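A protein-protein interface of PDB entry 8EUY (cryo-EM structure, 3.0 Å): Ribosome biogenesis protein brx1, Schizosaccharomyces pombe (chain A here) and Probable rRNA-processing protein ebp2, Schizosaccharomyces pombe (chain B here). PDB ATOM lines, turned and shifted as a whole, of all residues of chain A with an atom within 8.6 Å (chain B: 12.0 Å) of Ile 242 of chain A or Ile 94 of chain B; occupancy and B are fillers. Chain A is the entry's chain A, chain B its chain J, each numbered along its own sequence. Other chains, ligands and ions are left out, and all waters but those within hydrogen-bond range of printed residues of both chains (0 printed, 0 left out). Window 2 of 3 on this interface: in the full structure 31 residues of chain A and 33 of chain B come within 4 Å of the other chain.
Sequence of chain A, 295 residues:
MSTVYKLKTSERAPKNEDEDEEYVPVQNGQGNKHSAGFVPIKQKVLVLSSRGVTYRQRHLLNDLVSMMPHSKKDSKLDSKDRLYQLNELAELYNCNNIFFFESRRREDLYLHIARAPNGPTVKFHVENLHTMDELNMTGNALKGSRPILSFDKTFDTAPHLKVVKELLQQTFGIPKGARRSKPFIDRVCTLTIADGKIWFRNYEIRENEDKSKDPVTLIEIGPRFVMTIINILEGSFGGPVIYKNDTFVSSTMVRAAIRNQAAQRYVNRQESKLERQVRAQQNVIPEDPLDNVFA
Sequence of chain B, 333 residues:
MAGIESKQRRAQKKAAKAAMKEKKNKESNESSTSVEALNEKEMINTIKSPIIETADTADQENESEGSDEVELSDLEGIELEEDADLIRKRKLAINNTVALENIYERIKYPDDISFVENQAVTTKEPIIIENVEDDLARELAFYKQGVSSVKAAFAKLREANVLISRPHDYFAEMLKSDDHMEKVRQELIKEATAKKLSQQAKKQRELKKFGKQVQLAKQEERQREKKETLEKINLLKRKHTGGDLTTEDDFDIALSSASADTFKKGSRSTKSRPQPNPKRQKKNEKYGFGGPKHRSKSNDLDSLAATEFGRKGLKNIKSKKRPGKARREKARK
Of the 14 printed residues of chain B, 6 touch a printed residue of chain A. Of the 20 printed residues of chain A, 6 touch a printed residue of chain B. Hydrophobic or aromatic side chains of chain A within 4 Å of the printed part of chain B: Pro 159, Val 163 and Tyr 243. Among the printed residues, 10 pairs touch across the chains. Among the printed residues, no Asp or Glu carboxylate lies within 4 Å of a Lys or Arg side-chain nitrogen of the other chain.
Printed residues of chain B within 4 Å of His 160 of chain A: Leu 100 (3.9 Å). Printed residues of chain B within 4 Å of Val 163 of chain A: Leu 100 and Tyr 104. Ile 232 of chain A touches none of the printed residues of chain B. No residue of chain B comes within 4 Å of Leu 233 of chain A. No residue of chain B comes within 4 Å of Pro 240 of chain A. Of chain B, only Ile 94 (3.8 Å), Asn 95 (3.2 Å) and Asn 96 (3.0 Å) come within 4 Å of Ile 242 of chain A. Printed residues of chain B within 4 Å of Tyr 243 of chain A: Asn 95 (3.4 Å). Lys 244 of chain A touches just one residue of chain B: Asn 95. Of chain A, only Ile 242 (3.2 Å), Tyr 243 (3.4 Å) and Lys 244 (3.7 Å) come within 4 Å of Asn 95 of chain B. Of the printed residues of chain A, Thr 97 of chain B touches Pro 159.
NE2 of His 160 of chain A is in hydrogen-bond range of OH of Tyr 243 of chain A (3.2 Å). The backbone NH (N) of Ile 242 of chain A lies within hydrogen-bond range of the backbone carbonyl oxygen (O) of Ile 232 of chain A. The backbone NH (N) of Ile 232 of chain A lies within hydrogen-bond range of the backbone carbonyl oxygen (O) of Tyr 243 of chain A.
The backbone NH of Asn 95 of chain B sits at hydrogen-bond distance from the backbone carbonyl oxygen of Ile 242 of chain A. The backbone carbonyl oxygen of Ile 242 of chain A lies within hydrogen-bond range of the backbone NH of Asn 96 of chain B.
Pro 159 of chain A touches Thr 97 of chain B. Pro 159 of chain A touches Leu 100 of chain B. Leu 100 of chain B touches His 160 of chain A (CB to N, 3.9 Å). O of Leu 100 of chain B touches CG2 of Val 163 of chain A (3.3 Å). CG2 of Val 163 of chain A touches CB of Tyr 104 of chain B, at 3.7 Å. Ile 94 of chain B touches Ile 242 of chain A. CA of Tyr 243 of chain A touches N of Asn 95 of chain B, at 3.4 Å. Lys 244 of chain A touches Asn 95 of chain B.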
ATOM      1  N   GLY A 119       5.550   2.499   8.160  1.00  0.00           N
ATOM      2  CA  GLY A 119       4.710   2.585   9.338  1.00  0.00           C
ATOM      3  C   GLY A 119       3.253   2.895   9.059  1.00  0.00           C
ATOM      4  O   GLY A 119       2.869   3.253   7.947  1.00  0.00           O
ATOM      5  N   PRO A 120       2.394   2.772  10.094  1.00  0.00           N
ATOM      6  CA  PRO A 120       0.958   3.032   9.900  1.00  0.00           C
ATOM      7  C   PRO A 120       0.576   4.491  10.129  1.00  0.00           C
ATOM      8  O   PRO A 120       0.914   5.076  11.165  1.00  0.00           O
ATOM      9  CB  PRO A 120       0.304   2.112  10.930  1.00  0.00           C
ATOM     10  CG  PRO A 120       1.325   2.006  12.031  1.00  0.00           C
ATOM     11  CD  PRO A 120       2.686   2.310  11.457  1.00  0.00           C
ATOM     12  N   THR A 121      -0.132   5.084   9.175  1.00  0.00           N
ATOM     13  CA  THR A 121      -0.657   6.434   9.315  1.00  0.00           C
ATOM     14  C   THR A 121      -2.113   6.344   9.751  1.00  0.00           C
ATOM     15  O   THR A 121      -2.947   5.787   9.028  1.00  0.00           O
ATOM     16  CB  THR A 121      -0.546   7.217   8.004  1.00  0.00           C
ATOM     17  OG1 THR A 121       0.830   7.303   7.610  1.00  0.00           O
ATOM     18  CG2 THR A 121      -1.105   8.616   8.184  1.00  0.00           C
ATOM     19  N   PRO A 159      -7.478  -6.031  16.085  1.00  0.00           N
ATOM     20  CA  PRO A 159      -6.084  -5.798  15.671  1.00  0.00           C
ATOM     21  C   PRO A 159      -5.782  -4.346  15.348  1.00  0.00           C
ATOM     22  O   PRO A 159      -4.666  -3.883  15.616  1.00  0.00           O
ATOM     23  CB  PRO A 159      -5.930  -6.697  14.437  1.00  0.00           C
ATOM     24  CG  PRO A 159      -7.323  -6.918  13.945  1.00  0.00           C
ATOM     25  CD  PRO A 159      -8.177  -6.953  15.174  1.00  0.00           C
ATOM     26  N   HIS A 160      -6.739  -3.609  14.778  1.00  0.00           N
ATOM     27  CA  HIS A 160      -6.493  -2.204  14.472  1.00  0.00           C
ATOM     28  C   HIS A 160      -6.379  -1.376  15.746  1.00  0.00           C
ATOM     29  O   HIS A 160      -5.564  -0.449  15.819  1.00  0.00           O
ATOM     30  CB  HIS A 160      -7.594  -1.657  13.559  1.00  0.00           C
ATOM     31  CG  HIS A 160      -8.889  -1.386  14.259  1.00  0.00           C
ATOM     32  ND1 HIS A 160      -9.918  -2.302  14.304  1.00  0.00           N
ATOM     33  CD2 HIS A 160      -9.328  -0.296  14.932  1.00  0.00           C
ATOM     34  CE1 HIS A 160     -10.932  -1.791  14.979  1.00  0.00           C
ATOM     35  NE2 HIS A 160     -10.599  -0.575  15.371  1.00  0.00           N
ATOM     36  N   VAL A 163      -2.981  -1.889  17.125  1.00  0.00           N
ATOM     37  CA  VAL A 163      -1.970  -1.097  16.430  1.00  0.00           C
ATOM     38  C   VAL A 163      -1.954   0.330  16.960  1.00  0.00           C
ATOM     39  O   VAL A 163      -0.891   0.892  17.251  1.00  0.00           O
ATOM     40  CB  VAL A 163      -2.216  -1.132  14.911  1.00  0.00           C
ATOM     41  CG1 VAL A 163      -1.393  -0.063  14.212  1.00  0.00           C
ATOM     42  CG2 VAL A 163      -1.897  -2.507  14.355  1.00  0.00           C
ATOM     43  N   ASN A 231      -9.376   6.656   9.450  1.00  0.00           N
ATOM     44  CA  ASN A 231      -8.827   5.564   8.661  1.00  0.00           C
ATOM     45  C   ASN A 231      -7.367   5.375   9.040  1.00  0.00           C
ATOM     46  O   ASN A 231      -6.699   6.317   9.474  1.00  0.00           O
ATOM     47  CB  ASN A 231      -8.960   5.829   7.157  1.00  0.00           C
ATOM     48  CG  ASN A 231      -8.353   7.153   6.745  1.00  0.00           C
ATOM     49  OD1 ASN A 231      -8.499   8.158   7.441  1.00  0.00           O
ATOM     50  ND2 ASN A 231      -7.673   7.165   5.605  1.00  0.00           N
ATOM     51  N   ILE A 232      -6.882   4.148   8.874  1.00  0.00           N
ATOM     52  CA  ILE A 232      -5.500   3.795   9.171  1.00  0.00           C
ATOM     53  C   ILE A 232      -4.860   3.260   7.901  1.00  0.00           C
ATOM     54  O   ILE A 232      -5.408   2.361   7.253  1.00  0.00           O
ATOM     55  CB  ILE A 232      -5.408   2.764  10.311  1.00  0.00           C
ATOM     56  CG1 ILE A 232      -6.159   3.270  11.543  1.00  0.00           C
ATOM     57  CG2 ILE A 232      -3.955   2.472  10.648  1.00  0.00           C
ATOM     58  CD1 ILE A 232      -5.981   2.406  12.772  1.00  0.00           C
ATOM     59  N   LEU A 233      -3.708   3.814   7.544  1.00  0.00           N
ATOM     60  CA  LEU A 233      -2.981   3.415   6.350  1.00  0.00           C
ATOM     61  C   LEU A 233      -1.799   2.528   6.719  1.00  0.00           C
ATOM     62  O   LEU A 233      -1.447   2.367   7.889  1.00  0.00           O
ATOM     63  CB  LEU A 233      -2.509   4.647   5.571  1.00  0.00           C
ATOM     64  CG  LEU A 233      -3.443   5.860   5.578  1.00  0.00           C
ATOM     65  CD1 LEU A 233      -2.776   7.051   4.914  1.00  0.00           C
ATOM     66  CD2 LEU A 233      -4.753   5.532   4.885  1.00  0.00           C
ATOM     67  N   GLU A 234      -1.181   1.943   5.694  1.00  0.00           N
ATOM     68  CA  GLU A 234      -0.031   1.071   5.883  1.00  0.00           C
ATOM     69  C   GLU A 234       1.297   1.763   5.611  1.00  0.00           C
ATOM     70  O   GLU A 234       2.347   1.206   5.949  1.00  0.00           O
ATOM     71  CB  GLU A 234      -0.146  -0.166   4.983  1.00  0.00           C
ATOM     72  CG  GLU A 234       0.194   0.097   3.527  1.00  0.00           C
ATOM     73  CD  GLU A 234       0.273  -1.177   2.711  1.00  0.00           C
ATOM     74  OE1 GLU A 234      -0.042  -2.253   3.258  1.00  0.00           O
ATOM     75  OE2 GLU A 234       0.652  -1.101   1.523  1.00  0.00           O
ATOM     76  N   GLY A 235       1.280   2.956   5.011  1.00  0.00           N
ATOM     77  CA  GLY A 235       2.486   3.696   4.723  1.00  0.00           C
ATOM     78  C   GLY A 235       2.457   5.071   5.374  1.00  0.00           C
ATOM     79  O   GLY A 235       1.439   5.510   5.923  1.00  0.00           O
ATOM     80  N   GLY A 238       0.626   7.531   2.975  1.00  0.00           N
ATOM     81  CA  GLY A 238       0.495   6.987   1.637  1.00  0.00           C
ATOM     82  C   GLY A 238       0.180   5.511   1.698  1.00  0.00           C
ATOM     83  O   GLY A 238       0.058   4.919   2.773  1.00  0.00           O
ATOM     84  N   GLY A 239       0.047   4.919   0.514  1.00  0.00           N
ATOM     85  CA  GLY A 239      -0.286   3.521   0.396  1.00  0.00           C
ATOM     86  C   GLY A 239      -1.777   3.287   0.516  1.00  0.00           C
ATOM     87  O   GLY A 239      -2.541   4.183   0.888  1.00  0.00           O
ATOM     88  N   PRO A 240      -2.222   2.075   0.194  1.00  0.00           N
ATOM     89  CA  PRO A 240      -3.650   1.765   0.305  1.00  0.00           C
ATOM     90  C   PRO A 240      -4.119   1.795   1.750  1.00  0.00           C
ATOM     91  O   PRO A 240      -3.378   1.466   2.679  1.00  0.00           O
ATOM     92  CB  PRO A 240      -3.755   0.355  -0.285  1.00  0.00           C
ATOM     93  CG  PRO A 240      -2.390  -0.224  -0.127  1.00  0.00           C
ATOM     94  CD  PRO A 240      -1.434   0.923  -0.275  1.00  0.00           C
ATOM     95  N   VAL A 241      -5.376   2.199   1.931  1.00  0.00           N
ATOM     96  CA  VAL A 241      -5.965   2.234   3.264  1.00  0.00           C
ATOM     97  C   VAL A 241      -6.296   0.815   3.703  1.00  0.00           C
ATOM     98  O   VAL A 241      -6.929   0.048   2.964  1.00  0.00           O
ATOM     99  CB  VAL A 241      -7.208   3.137   3.282  1.00  0.00           C
ATOM    100  CG1 VAL A 241      -8.126   2.815   2.111  1.00  0.00           C
ATOM    101  CG2 VAL A 241      -7.948   2.996   4.602  1.00  0.00           C
ATOM    102  N   ILE A 242      -5.855   0.450   4.906  1.00  0.00           N
ATOM    103  CA  ILE A 242      -6.055  -0.905   5.404  1.00  0.00           C
ATOM    104  C   ILE A 242      -7.210  -1.011   6.395  1.00  0.00           C
ATOM    105  O   ILE A 242      -7.737  -2.116   6.593  1.00  0.00           O
ATOM    106  CB  ILE A 242      -4.762  -1.453   6.042  1.00  0.00           C
ATOM    107  CG1 ILE A 242      -4.452  -0.721   7.348  1.00  0.00           C
ATOM    108  CG2 ILE A 242      -3.602  -1.333   5.067  1.00  0.00           C
ATOM    109  CD1 ILE A 242      -3.418  -1.415   8.203  1.00  0.00           C
ATOM    110  N   TYR A 243      -7.620   0.092   7.018  1.00  0.00           N
ATOM    111  CA  TYR A 243      -8.722   0.065   7.968  1.00  0.00           C
ATOM    112  C   TYR A 243      -9.576   1.309   7.791  1.00  0.00           C
ATOM    113  O   TYR A 243      -9.056   2.427   7.783  1.00  0.00           O
ATOM    114  CB  TYR A 243      -8.214  -0.027   9.413  1.00  0.00           C
ATOM    115  CG  TYR A 243      -9.247   0.347  10.455  1.00  0.00           C
ATOM    116  CD1 TYR A 243     -10.128  -0.602  10.954  1.00  0.00           C
ATOM    117  CD2 TYR A 243      -9.327   1.641  10.954  1.00  0.00           C
ATOM    118  CE1 TYR A 243     -11.071  -0.269  11.906  1.00  0.00           C
ATOM    119  CE2 TYR A 243     -10.268   1.982  11.906  1.00  0.00           C
ATOM    120  CZ  TYR A 243     -11.135   1.022  12.380  1.00  0.00           C
ATOM    121  OH  TYR A 243     -12.071   1.356  13.330  1.00  0.00           O
ATOM    122  N   LYS A 244     -10.882   1.107   7.657  1.00  0.00           N
ATOM    123  CA  LYS A 244     -11.857   2.188   7.644  1.00  0.00           C
ATOM    124  C   LYS A 244     -12.757   2.043   8.862  1.00  0.00           C
ATOM    125  O   LYS A 244     -13.307   0.964   9.105  1.00  0.00           O
ATOM    126  CB  LYS A 244     -12.687   2.169   6.359  1.00  0.00           C
ATOM    127  CG  LYS A 244     -13.553   3.401   6.171  1.00  0.00           C
ATOM    128  CD  LYS A 244     -12.739   4.573   5.658  1.00  0.00           C
ATOM    129  CE  LYS A 244     -13.569   5.845   5.618  1.00  0.00           C
ATOM    130  NZ  LYS A 244     -14.658   5.768   4.604  1.00  0.00           N
ATOM    131  N   ASN A 245     -12.897   3.127   9.627  1.00  0.00           N
ATOM    132  CA  ASN A 245     -13.650   3.057  10.875  1.00  0.00           C
ATOM    133  C   ASN A 245     -15.113   2.720  10.625  1.00  0.00           C
ATOM    134  O   ASN A 245     -15.718   1.949  11.380  1.00  0.00           O
ATOM    135  CB  ASN A 245     -13.525   4.375  11.637  1.00  0.00           C
ATOM    136  CG  ASN A 245     -13.600   4.186  13.136  1.00  0.00           C
ATOM    137  OD1 ASN A 245     -12.879   3.368  13.708  1.00  0.00           O
ATOM    138  ND2 ASN A 245     -14.468   4.951  13.785  1.00  0.00           N
ATOM    139  N   ASP A 246     -15.704   3.302   9.579  1.00  0.00           N
ATOM    140  CA  ASP A 246     -17.093   3.065   9.189  1.00  0.00           C
ATOM    141  C   ASP A 246     -18.085   3.465  10.278  1.00  0.00           C
ATOM    142  O   ASP A 246     -19.251   3.059  10.235  1.00  0.00           O
ATOM    143  CB  ASP A 246     -17.316   1.603   8.782  1.00  0.00           C
ATOM    144  CG  ASP A 246     -18.410   1.449   7.744  1.00  0.00           C
ATOM    145  OD1 ASP A 246     -18.937   2.480   7.278  1.00  0.00           O
ATOM    146  OD2 ASP A 246     -18.742   0.296   7.394  1.00  0.00           O
ATOM    147  N   ILE B  94     -10.912  -2.797   4.057  1.00  0.00           N
ATOM    148  CA  ILE B  94     -11.506  -2.174   5.233  1.00  0.00           C
ATOM    149  C   ILE B  94     -11.421  -3.114   6.427  1.00  0.00           C
ATOM    150  O   ILE B  94     -11.903  -4.246   6.370  1.00  0.00           O
ATOM    151  CB  ILE B  94     -12.964  -1.760   4.967  1.00  0.00           C
ATOM    152  N   ASN B  95     -10.806  -2.630   7.509  1.00  0.00           N
ATOM    153  CA  ASN B  95     -10.632  -3.401   8.740  1.00  0.00           C
ATOM    154  C   ASN B  95      -9.925  -4.728   8.468  1.00  0.00           C
ATOM    155  O   ASN B  95     -10.335  -5.790   8.942  1.00  0.00           O
ATOM    156  CB  ASN B  95     -11.974  -3.626   9.442  1.00  0.00           C
ATOM    157  N   ASN B  96      -8.847  -4.661   7.689  1.00  0.00           N
ATOM    158  CA  ASN B  96      -8.071  -5.849   7.349  1.00  0.00           C
ATOM    159  C   ASN B  96      -7.353  -6.359   8.594  1.00  0.00           C
ATOM    160  O   ASN B  96      -6.367  -5.764   9.039  1.00  0.00           O
ATOM    161  CB  ASN B  96      -7.078  -5.530   6.236  1.00  0.00           C
ATOM    162  N   THR B  97      -7.853  -7.460   9.159  1.00  0.00           N
ATOM    163  CA  THR B  97      -7.243  -8.020  10.362  1.00  0.00           C
ATOM    164  C   THR B  97      -5.834  -8.530  10.087  1.00  0.00           C
ATOM    165  O   THR B  97      -4.932  -8.348  10.913  1.00  0.00           O
ATOM    166  CB  THR B  97      -8.117  -9.142  10.922  1.00  0.00           C
ATOM    167  N   VAL B  98      -5.628  -9.180   8.939  1.00  0.00           N
ATOM    168  CA  VAL B  98      -4.310  -9.716   8.612  1.00  0.00           C
ATOM    169  C   VAL B  98      -3.298  -8.588   8.453  1.00  0.00           C
ATOM    170  O   VAL B  98      -2.170  -8.671   8.952  1.00  0.00           O
ATOM    171  CB  VAL B  98      -4.387 -10.589   7.347  1.00  0.00           C
ATOM    172  N   ALA B  99      -3.682  -7.520   7.749  1.00  0.00           N
ATOM    173  CA  ALA B  99      -2.778  -6.392   7.564  1.00  0.00           C
ATOM    174  C   ALA B  99      -2.464  -5.711   8.890  1.00  0.00           C
ATOM    175  O   ALA B  99      -1.311  -5.349   9.154  1.00  0.00           O
ATOM    176  CB  ALA B  99      -3.379  -5.393   6.576  1.00  0.00           C
ATOM    177  N   LEU B 100      -3.478  -5.524   9.738  1.00  0.00           N
ATOM    178  CA  LEU B 100      -3.253  -4.895  11.035  1.00  0.00           C
ATOM    179  C   LEU B 100      -2.353  -5.754  11.915  1.00  0.00           C
ATOM    180  O   LEU B 100      -1.482  -5.233  12.622  1.00  0.00           O
ATOM    181  CB  LEU B 100      -4.587  -4.628  11.728  1.00  0.00           C
ATOM    182  N   GLU B 101      -2.553  -7.074  11.891  1.00  0.00           N
ATOM    183  CA  GLU B 101      -1.711  -7.964  12.685  1.00  0.00           C
ATOM    184  C   GLU B 101      -0.259  -7.901  12.231  1.00  0.00           C
ATOM    185  O   GLU B 101       0.660  -7.889  13.059  1.00  0.00           O
ATOM    186  CB  GLU B 101      -2.239  -9.396  12.603  1.00  0.00           C
ATOM    187  N   ASN B 102      -0.030  -7.864  10.916  1.00  0.00           N
ATOM    188  CA  ASN B 102       1.332  -7.740  10.406  1.00  0.00           C
ATOM    189  C   ASN B 102       1.947  -6.404  10.802  1.00  0.00           C
ATOM    190  O   ASN B 102       3.127  -6.337  11.165  1.00  0.00           O
ATOM    191  CB  ASN B 102       1.342  -7.909   8.887  1.00  0.00           C
ATOM    192  N   ILE B 103       1.163  -5.327  10.731  1.00  0.00           N
ATOM    193  CA  ILE B 103       1.659  -4.016  11.141  1.00  0.00           C
ATOM    194  C   ILE B 103       1.953  -3.999  12.634  1.00  0.00           C
ATOM    195  O   ILE B 103       2.955  -3.422  13.075  1.00  0.00           O
ATOM    196  CB  ILE B 103       0.654  -2.918  10.748  1.00  0.00           C
ATOM    197  N   TYR B 104       1.084  -4.618  13.437  1.00  0.00           N
ATOM    198  CA  TYR B 104       1.316  -4.674  14.876  1.00  0.00           C
ATOM    199  C   TYR B 104       2.592  -5.441  15.198  1.00  0.00           C
ATOM    200  O   TYR B 104       3.375  -5.024  16.058  1.00  0.00           O
ATOM    201  CB  TYR B 104       0.117  -5.311  15.578  1.00  0.00           C
ATOM    202  N   GLU B 105       2.816  -6.569  14.520  1.00  0.00           N
ATOM    203  CA  GLU B 105       4.032  -7.343  14.746  1.00  0.00           C
ATOM    204  C   GLU B 105       5.273  -6.570  14.318  1.00  0.00           C
ATOM    205  O   GLU B 105       6.304  -6.615  14.998  1.00  0.00           O
ATOM    206  CB  GLU B 105       3.949  -8.678  14.006  1.00  0.00           C
ATOM    207  N   ARG B 106       5.194  -5.861  13.189  1.00  0.00           N
ATOM    208  CA  ARG B 106       6.350  -5.121  12.693  1.00  0.00           C
ATOM    209  C   ARG B 106       6.739  -3.991  13.638  1.00  0.00           C
ATOM    210  O   ARG B 106       7.931  -3.732  13.847  1.00  0.00           O
ATOM    211  CB  ARG B 106       6.061  -4.574  11.295  1.00  0.00           C
ATOM    212  N   ILE B 107       5.754  -3.308  14.220  1.00  0.00           N
ATOM    213  CA  ILE B 107       6.020  -2.154  15.071  1.00  0.00           C
ATOM    214  C   ILE B 107       5.780  -2.516  16.530  1.00  0.00           C
ATOM    215  O   ILE B 107       5.481  -1.645  17.355  1.00  0.00           O
ATOM    216  CB  ILE B 107       5.155  -0.950  14.655  1.00  0.00           C
